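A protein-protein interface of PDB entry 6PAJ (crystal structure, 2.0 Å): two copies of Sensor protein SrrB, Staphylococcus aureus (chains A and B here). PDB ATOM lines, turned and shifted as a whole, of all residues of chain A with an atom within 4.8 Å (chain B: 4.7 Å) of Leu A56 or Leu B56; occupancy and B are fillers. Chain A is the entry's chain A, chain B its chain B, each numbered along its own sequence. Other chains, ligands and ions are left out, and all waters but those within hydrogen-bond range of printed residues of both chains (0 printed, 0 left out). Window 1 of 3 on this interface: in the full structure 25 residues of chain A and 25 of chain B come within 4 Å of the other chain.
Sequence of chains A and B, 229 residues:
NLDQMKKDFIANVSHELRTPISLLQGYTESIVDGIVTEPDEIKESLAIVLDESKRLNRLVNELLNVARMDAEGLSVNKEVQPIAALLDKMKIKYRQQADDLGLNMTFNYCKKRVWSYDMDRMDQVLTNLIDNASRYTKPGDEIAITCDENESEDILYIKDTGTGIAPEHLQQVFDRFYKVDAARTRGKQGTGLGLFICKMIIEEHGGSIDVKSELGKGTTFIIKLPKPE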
ATOM      1  N   LEU A  17       6.113  13.135 -20.942  1.00  0.00           N
ATOM      2  CA  LEU A  17       6.574  12.290 -22.030  1.00  0.00           C
ATOM      3  C   LEU A  17       6.423  13.025 -23.374  1.00  0.00           C
ATOM      4  O   LEU A  17       7.290  12.883 -24.244  1.00  0.00           O
ATOM      5  CB  LEU A  17       5.824  10.961 -22.037  1.00  0.00           C
ATOM      6  CG  LEU A  17       6.179  10.019 -20.885  1.00  0.00           C
ATOM      7  CD1 LEU A  17       5.084   8.995 -20.709  1.00  0.00           C
ATOM      8  CD2 LEU A  17       7.530   9.373 -21.138  1.00  0.00           C
ATOM      9  N   PRO A  20       9.739  15.384 -24.876  1.00  0.00           N
ATOM     10  CA  PRO A  20      10.865  14.726 -25.532  1.00  0.00           C
ATOM     11  C   PRO A  20      10.456  14.005 -26.827  1.00  0.00           C
ATOM     12  O   PRO A  20      11.202  14.108 -27.793  1.00  0.00           O
ATOM     13  CB  PRO A  20      11.464  13.740 -24.514  1.00  0.00           C
ATOM     14  CG  PRO A  20      10.413  13.671 -23.422  1.00  0.00           C
ATOM     15  CD  PRO A  20       9.764  15.040 -23.438  1.00  0.00           C
ATOM     16  N   ILE A  21       9.286  13.367 -26.865  1.00  0.00           N
ATOM     17  CA  ILE A  21       8.838  12.643 -28.053  1.00  0.00           C
ATOM     18  C   ILE A  21       8.618  13.643 -29.198  1.00  0.00           C
ATOM     19  O   ILE A  21       8.967  13.345 -30.354  1.00  0.00           O
ATOM     20  CB  ILE A  21       7.570  11.822 -27.755  1.00  0.00           C
ATOM     21  CG1 ILE A  21       7.888  10.639 -26.832  1.00  0.00           C
ATOM     22  CG2 ILE A  21       6.901  11.362 -29.043  1.00  0.00           C
ATOM     23  CD1 ILE A  21       6.671  10.009 -26.222  1.00  0.00           C
ATOM     24  N   LEU A  24      12.154  14.729 -30.458  1.00  0.00           N
ATOM     25  CA  LEU A  24      12.811  13.678 -31.234  1.00  0.00           C
ATOM     26  C   LEU A  24      12.255  13.692 -32.658  1.00  0.00           C
ATOM     27  O   LEU A  24      13.026  13.742 -33.614  1.00  0.00           O
ATOM     28  CB  LEU A  24      12.527  12.300 -30.636  1.00  0.00           C
ATOM     29  CG  LEU A  24      13.147  11.979 -29.281  1.00  0.00           C
ATOM     30  CD1 LEU A  24      12.635  10.633 -28.799  1.00  0.00           C
ATOM     31  CD2 LEU A  24      14.650  12.007 -29.352  1.00  0.00           C
ATOM     32  N   GLU A  52      17.418  14.135 -25.701  1.00  0.00           N
ATOM     33  CA  GLU A  52      16.000  13.907 -25.419  1.00  0.00           C
ATOM     34  C   GLU A  52      15.700  12.400 -25.391  1.00  0.00           C
ATOM     35  O   GLU A  52      14.820  11.973 -24.659  1.00  0.00           O
ATOM     36  CB  GLU A  52      15.103  14.641 -26.418  1.00  0.00           C
ATOM     37  CG  GLU A  52      15.146  16.180 -26.318  1.00  0.00           C
ATOM     38  CD  GLU A  52      14.877  16.760 -24.943  1.00  0.00           C
ATOM     39  OE1 GLU A  52      15.540  17.735 -24.584  1.00  0.00           O
ATOM     40  OE2 GLU A  52      14.007  16.228 -24.236  1.00  0.00           O
ATOM     41  N   SER A  53      16.417  11.594 -26.163  1.00  0.00           N
ATOM     42  CA  SER A  53      16.192  10.153 -26.130  1.00  0.00           C
ATOM     43  C   SER A  53      16.559   9.585 -24.744  1.00  0.00           C
ATOM     44  O   SER A  53      15.836   8.730 -24.242  1.00  0.00           O
ATOM     45  CB  SER A  53      16.903   9.439 -27.261  1.00  0.00           C
ATOM     46  OG  SER A  53      18.311   9.389 -27.088  1.00  0.00           O
ATOM     47  N   LYS A  54      17.650  10.083 -24.158  1.00  0.00           N
ATOM     48  CA  LYS A  54      18.092   9.727 -22.807  1.00  0.00           C
ATOM     49  C   LYS A  54      17.075  10.177 -21.780  1.00  0.00           C
ATOM     50  O   LYS A  54      16.741   9.399 -20.897  1.00  0.00           O
ATOM     51  CB  LYS A  54      19.432  10.379 -22.486  1.00  0.00           C
ATOM     52  CG  LYS A  54      20.570   9.758 -23.253  1.00  0.00           C
ATOM     53  CD  LYS A  54      21.915  10.313 -22.909  1.00  0.00           C
ATOM     54  CE  LYS A  54      23.021   9.548 -23.606  1.00  0.00           C
ATOM     55  NZ  LYS A  54      23.925  10.499 -24.296  1.00  0.00           N
ATOM     56  N   ARG A  55      16.583  11.420 -21.898  1.00  0.00           N
ATOM     57  CA  ARG A  55      15.544  11.890 -20.996  1.00  0.00           C
ATOM     58  C   ARG A  55      14.305  10.983 -21.071  1.00  0.00           C
ATOM     59  O   ARG A  55      13.735  10.609 -20.035  1.00  0.00           O
ATOM     60  CB  ARG A  55      15.220  13.360 -21.278  1.00  0.00           C
ATOM     61  CG  ARG A  55      14.174  13.978 -20.356  1.00  0.00           C
ATOM     62  CD  ARG A  55      13.724  15.381 -20.790  1.00  0.00           C
ATOM     63  NE  ARG A  55      14.537  16.446 -20.213  1.00  0.00           N
ATOM     64  CZ  ARG A  55      15.676  16.935 -20.721  1.00  0.00           C
ATOM     65  NH1 ARG A  55      16.179  16.458 -21.845  1.00  0.00           N
ATOM     66  NH2 ARG A  55      16.301  17.926 -20.101  1.00  0.00           N
ATOM     67  N   LEU A  56      13.860  10.641 -22.273  1.00  0.00           N
ATOM     68  CA  LEU A  56      12.678   9.813 -22.476  1.00  0.00           C
ATOM     69  C   LEU A  56      12.842   8.448 -21.775  1.00  0.00           C
ATOM     70  O   LEU A  56      11.909   7.925 -21.176  1.00  0.00           O
ATOM     71  CB  LEU A  56      12.530   9.584 -23.992  1.00  0.00           C
ATOM     72  CG  LEU A  56      11.137   9.420 -24.590  1.00  0.00           C
ATOM     73  CD1 LEU A  56      11.124   8.373 -25.698  1.00  0.00           C
ATOM     74  CD2 LEU A  56      10.053   9.134 -23.570  1.00  0.00           C
ATOM     75  N   ASN A  57      14.016   7.859 -21.965  1.00  0.00           N
ATOM     76  CA  ASN A  57      14.355   6.542 -21.435  1.00  0.00           C
ATOM     77  C   ASN A  57      14.258   6.581 -19.906  1.00  0.00           C
ATOM     78  O   ASN A  57      13.632   5.708 -19.303  1.00  0.00           O
ATOM     79  CB  ASN A  57      15.745   6.092 -21.897  1.00  0.00           C
ATOM     80  CG  ASN A  57      15.953   4.606 -21.705  1.00  0.00           C
ATOM     81  OD1 ASN A  57      15.110   3.798 -22.081  1.00  0.00           O
ATOM     82  ND2 ASN A  57      17.061   4.242 -21.100  1.00  0.00           N
ATOM     83  N   ARG A  58      14.837   7.627 -19.308  1.00  0.00           N
ATOM     84  CA  ARG A  58      14.813   7.773 -17.846  1.00  0.00           C
ATOM     85  C   ARG A  58      13.368   7.873 -17.381  1.00  0.00           C
ATOM     86  O   ARG A  58      12.990   7.275 -16.366  1.00  0.00           O
ATOM     87  CB  ARG A  58      15.590   9.011 -17.378  1.00  0.00           C
ATOM     88  CG  ARG A  58      17.098   8.881 -17.521  1.00  0.00           C
ATOM     89  CD  ARG A  58      17.845   9.919 -16.696  1.00  0.00           C
ATOM     90  NE  ARG A  58      17.626  11.272 -17.203  1.00  0.00           N
ATOM     91  CZ  ARG A  58      18.309  11.828 -18.206  1.00  0.00           C
ATOM     92  NH1 ARG A  58      19.336  11.208 -18.754  1.00  0.00           N
ATOM     93  NH2 ARG A  58      17.973  13.023 -18.638  1.00  0.00           N
ATOM     94  N   LEU A  59      12.566   8.623 -18.134  1.00  0.00           N
ATOM     95  CA  LEU A  59      11.197   8.847 -17.741  1.00  0.00           C
ATOM     96  C   LEU A  59      10.394   7.552 -17.864  1.00  0.00           C
ATOM     97  O   LEU A  59       9.464   7.299 -17.070  1.00  0.00           O
ATOM     98  CB  LEU A  59      10.542   9.925 -18.617  1.00  0.00           C
ATOM     99  CG  LEU A  59      10.933  11.364 -18.291  1.00  0.00           C
ATOM    100  CD1 LEU A  59      10.577  12.300 -19.453  1.00  0.00           C
ATOM    101  CD2 LEU A  59      10.278  11.826 -16.985  1.00  0.00           C
ATOM    102  N   VAL A  60      10.638   6.841 -18.954  1.00  0.00           N
ATOM    103  CA  VAL A  60       9.894   5.599 -19.215  1.00  0.00           C
ATOM    104  C   VAL A  60      10.208   4.585 -18.091  1.00  0.00           C
ATOM    105  O   VAL A  60       9.286   4.025 -17.508  1.00  0.00           O
ATOM    106  CB  VAL A  60      10.206   5.043 -20.611  1.00  0.00           C
ATOM    107  CG1 VAL A  60       9.870   3.571 -20.724  1.00  0.00           C
ATOM    108  CG2 VAL A  60       9.508   5.855 -21.705  1.00  0.00           C
ATOM    109  N   LEU B  17       8.728  -0.500 -25.515  1.00  0.00           N
ATOM    110  CA  LEU B  17       9.163   0.885 -25.497  1.00  0.00           C
ATOM    111  C   LEU B  17      10.707   0.975 -25.518  1.00  0.00           C
ATOM    112  O   LEU B  17      11.282   1.903 -26.093  1.00  0.00           O
ATOM    113  CB  LEU B  17       8.633   1.577 -24.247  1.00  0.00           C
ATOM    114  CG  LEU B  17       7.126   1.850 -24.170  1.00  0.00           C
ATOM    115  CD1 LEU B  17       6.802   2.465 -22.823  1.00  0.00           C
ATOM    116  CD2 LEU B  17       6.678   2.794 -25.270  1.00  0.00           C
ATOM    117  N   PRO B  20      12.495   0.481 -29.370  1.00  0.00           N
ATOM    118  CA  PRO B  20      12.579   1.634 -30.267  1.00  0.00           C
ATOM    119  C   PRO B  20      13.521   2.711 -29.702  1.00  0.00           C
ATOM    120  O   PRO B  20      14.248   3.331 -30.466  1.00  0.00           O
ATOM    121  CB  PRO B  20      11.140   2.158 -30.488  1.00  0.00           C
ATOM    122  CG  PRO B  20      10.308   1.447 -29.456  1.00  0.00           C
ATOM    123  CD  PRO B  20      11.065   0.169 -29.161  1.00  0.00           C
ATOM    124  N   ILE B  21      13.581   2.875 -28.383  1.00  0.00           N
ATOM    125  CA  ILE B  21      14.491   3.862 -27.833  1.00  0.00           C
ATOM    126  C   ILE B  21      15.947   3.427 -28.118  1.00  0.00           C
ATOM    127  O   ILE B  21      16.777   4.221 -28.573  1.00  0.00           O
ATOM    128  CB  ILE B  21      14.215   4.090 -26.332  1.00  0.00           C
ATOM    129  CG1 ILE B  21      12.865   4.773 -26.112  1.00  0.00           C
ATOM    130  CG2 ILE B  21      15.340   4.883 -25.706  1.00  0.00           C
ATOM    131  CD1 ILE B  21      12.350   4.645 -24.700  1.00  0.00           C
ATOM    132  N   LEU B  24      16.780   4.088 -31.918  1.00  0.00           N
ATOM    133  CA  LEU B  24      17.012   5.453 -32.397  1.00  0.00           C
ATOM    134  C   LEU B  24      18.196   6.086 -31.656  1.00  0.00           C
ATOM    135  O   LEU B  24      18.918   6.880 -32.230  1.00  0.00           O
ATOM    136  CB  LEU B  24      15.715   6.258 -32.280  1.00  0.00           C
ATOM    137  CG  LEU B  24      15.378   6.827 -30.920  1.00  0.00           C
ATOM    138  CD1 LEU B  24      16.097   8.155 -30.738  1.00  0.00           C
ATOM    139  CD2 LEU B  24      13.857   6.971 -30.769  1.00  0.00           C
ATOM    140  N   GLU B  52      11.141   5.214 -35.762  1.00  0.00           N
ATOM    141  CA  GLU B  52      11.115   4.755 -34.370  1.00  0.00           C
ATOM    142  C   GLU B  52      10.515   5.825 -33.434  1.00  0.00           C
ATOM    143  O   GLU B  52       9.747   5.462 -32.494  1.00  0.00           O
ATOM    144  CB  GLU B  52      12.521   4.329 -33.943  1.00  0.00           C
ATOM    145  CG  GLU B  52      13.022   3.069 -34.678  1.00  0.00           C
ATOM    146  CD  GLU B  52      12.127   1.846 -34.656  1.00  0.00           C
ATOM    147  OE1 GLU B  52      12.015   1.164 -35.686  1.00  0.00           O
ATOM    148  OE2 GLU B  52      11.519   1.586 -33.635  1.00  0.00           O
ATOM    149  N   SER B  53      10.786   7.113 -33.707  1.00  0.00           N
ATOM    150  CA  SER B  53      10.227   8.185 -32.927  1.00  0.00           C
ATOM    151  C   SER B  53       8.694   8.200 -33.100  1.00  0.00           C
ATOM    152  O   SER B  53       7.973   8.371 -32.104  1.00  0.00           O
ATOM    153  CB  SER B  53      10.815   9.520 -33.286  1.00  0.00           C
ATOM    154  OG  SER B  53      12.235   9.547 -33.116  1.00  0.00           O
ATOM    155  N   LYS B  54       8.202   7.993 -34.316  1.00  0.00           N
ATOM    156  CA  LYS B  54       6.753   7.997 -34.563  1.00  0.00           C
ATOM    157  C   LYS B  54       6.121   6.761 -33.916  1.00  0.00           C
ATOM    158  O   LYS B  54       5.030   6.845 -33.366  1.00  0.00           O
ATOM    159  CB  LYS B  54       6.419   7.990 -36.050  1.00  0.00           C
ATOM    160  CG  LYS B  54       6.780   9.265 -36.791  1.00  0.00           C
ATOM    161  CD  LYS B  54       6.509   9.161 -38.256  1.00  0.00           C
ATOM    162  CE  LYS B  54       6.975  10.388 -39.015  1.00  0.00           C
ATOM    163  NZ  LYS B  54       6.911  10.141 -40.480  1.00  0.00           N
ATOM    164  N   ARG B  55       6.806   5.613 -33.987  1.00  0.00           N
ATOM    165  CA  ARG B  55       6.304   4.392 -33.384  1.00  0.00           C
ATOM    166  C   ARG B  55       6.215   4.535 -31.857  1.00  0.00           C
ATOM    167  O   ARG B  55       5.290   4.002 -31.209  1.00  0.00           O
ATOM    168  CB  ARG B  55       7.202   3.218 -33.789  1.00  0.00           C
ATOM    169  CG  ARG B  55       6.958   1.951 -32.992  1.00  0.00           C
ATOM    170  CD  ARG B  55       7.809   0.787 -33.474  1.00  0.00           C
ATOM    171  NE  ARG B  55       7.271   0.188 -34.688  1.00  0.00           N
ATOM    172  CZ  ARG B  55       7.616   0.528 -35.933  1.00  0.00           C
ATOM    173  NH1 ARG B  55       8.684   1.274 -36.154  1.00  0.00           N
ATOM    174  NH2 ARG B  55       6.886   0.119 -36.958  1.00  0.00           N
ATOM    175  N   LEU B  56       7.205   5.201 -31.261  1.00  0.00           N
ATOM    176  CA  LEU B  56       7.228   5.448 -29.836  1.00  0.00           C
ATOM    177  C   LEU B  56       6.047   6.314 -29.433  1.00  0.00           C
ATOM    178  O   LEU B  56       5.469   6.044 -28.413  1.00  0.00           O
ATOM    179  CB  LEU B  56       8.491   6.207 -29.430  1.00  0.00           C
ATOM    180  CG  LEU B  56       9.645   5.342 -29.003  1.00  0.00           C
ATOM    181  CD1 LEU B  56      10.915   6.170 -28.923  1.00  0.00           C
ATOM    182  CD2 LEU B  56       9.305   4.675 -27.670  1.00  0.00           C
ATOM    183  N   ASN B  57       5.784   7.378 -30.195  1.00  0.00           N
ATOM    184  CA  ASN B  57       4.655   8.245 -29.897  1.00  0.00           C
ATOM    185  C   ASN B  57       3.361   7.407 -29.862  1.00  0.00           C
ATOM    186  O   ASN B  57       2.541   7.592 -28.977  1.00  0.00           O
ATOM    187  CB  ASN B  57       4.576   9.435 -30.859  1.00  0.00           C
ATOM    188  CG  ASN B  57       3.448  10.399 -30.516  1.00  0.00           C
ATOM    189  OD1 ASN B  57       2.630  10.742 -31.365  1.00  0.00           O
ATOM    190  ND2 ASN B  57       3.336  10.774 -29.261  1.00  0.00           N
ATOM    191  N   ARG B  58       3.185   6.493 -30.814  1.00  0.00           N
ATOM    192  CA  ARG B  58       1.956   5.710 -30.951  1.00  0.00           C
ATOM    193  C   ARG B  58       1.865   4.738 -29.775  1.00  0.00           C
ATOM    194  O   ARG B  58       0.792   4.574 -29.184  1.00  0.00           O
ATOM    195  CB  ARG B  58       1.944   4.942 -32.279  1.00  0.00           C
ATOM    196  CG  ARG B  58       1.833   5.853 -33.503  1.00  0.00           C
ATOM    197  CD  ARG B  58       1.363   5.068 -34.700  1.00  0.00           C
ATOM    198  NE  ARG B  58       2.273   4.015 -35.093  1.00  0.00           N
ATOM    199  CZ  ARG B  58       3.372   4.202 -35.839  1.00  0.00           C
ATOM    200  NH1 ARG B  58       3.632   5.382 -36.363  1.00  0.00           N
ATOM    201  NH2 ARG B  58       4.168   3.190 -36.104  1.00  0.00           N
ATOM    202  N   LEU B  59       2.994   4.119 -29.448  1.00  0.00           N
ATOM    203  CA  LEU B  59       3.055   3.178 -28.307  1.00  0.00           C
ATOM    204  C   LEU B  59       2.764   3.911 -26.994  1.00  0.00           C
ATOM    205  O   LEU B  59       1.994   3.393 -26.143  1.00  0.00           O
ATOM    206  CB  LEU B  59       4.435   2.505 -28.231  1.00  0.00           C
ATOM    207  CG  LEU B  59       4.777   1.512 -29.337  1.00  0.00           C
ATOM    208  CD1 LEU B  59       6.246   1.092 -29.278  1.00  0.00           C
ATOM    209  CD2 LEU B  59       3.899   0.281 -29.267  1.00  0.00           C
ATOM    210  N   VAL B  60       3.378   5.078 -26.799  1.00  0.00           N
ATOM    211  CA  VAL B  60       3.160   5.820 -25.568  1.00  0.00           C
ATOM    212  C   VAL B  60       1.683   6.262 -25.432  1.00  0.00           C
ATOM    213  O   VAL B  60       1.067   6.097 -24.365  1.00  0.00           O
ATOM    214  CB  VAL B  60       4.143   6.993 -25.445  1.00  0.00           C
ATOM    215  CG1 VAL B  60       3.785   7.890 -24.273  1.00  0.00           C
ATOM    216  CG2 VAL B  60       5.582   6.467 -25.308  1.00  0.00           C
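Hydrophobic or aromatic side chains of chain B that line the printed part of chain A: Leu B17, Ile B21, Leu B24, Leu B56 and Val B60. Of the 13 printed residues of chain A, 7 touch a printed residue of chain B. Hydrophobic or aromatic side chains of chain A that line the printed part of chain B: Leu A17, Ile A21, Leu A24, Leu A56 and Val A60.
CD1 of Leu A17 touches CG1 of Val B60, 3.95 Å away. CG2 of Ile A21 touches CB of Asn B57, at 3.5 Å. Val B60 touches Ile A21 (CG2 to CD1, 3.8 Å). CB of Leu A24 touches OG of Ser B53, at 3.7 Å. Ser A53 touches Leu B24 (CB to CD1, 3.8 Å). Leu A56 touches Leu B56. OD1 of Asn A57 touches CG2 of Ile B21 (3.8 Å). Leu B17 touches Val A60.
Leu A17 touches Val B60, and with the chains exchanged Val A60 touches Leu B17. Ile A21 touches Asn B57, and with the chains exchanged Asn A57 touches Ile B21. Ile A21 touches Val B60, but with the chains exchanged Val A60 does not touch Ile B21 (4.3 Å). Leu A24 touches Ser B53, and with the chains exchanged Ser A53 touches Leu B24. 13 positions are printed for both chains. Of the 8 pairs that touch across the chains among the printed residues, 7 have their exchanged pair printed and touching as well.
Printed residues of chain B within 4 Å of Ile A21: Asn B57 (3.5 Å) and Val B60 (3.8 Å). Leu A56 touches just one residue of chain B: Leu B56. Of the printed residues of chain A, Ser B53 touches Leu A24 (3.7 Å). Lys B54 touches none of the printed residues of chain A. The nearest residue of chain B that does not touch Leu A56 is Ile B21 (4.02 Å). The nearest printed residue of chain A that does not touch Leu B56 is Ile A21 (4.7 Å).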
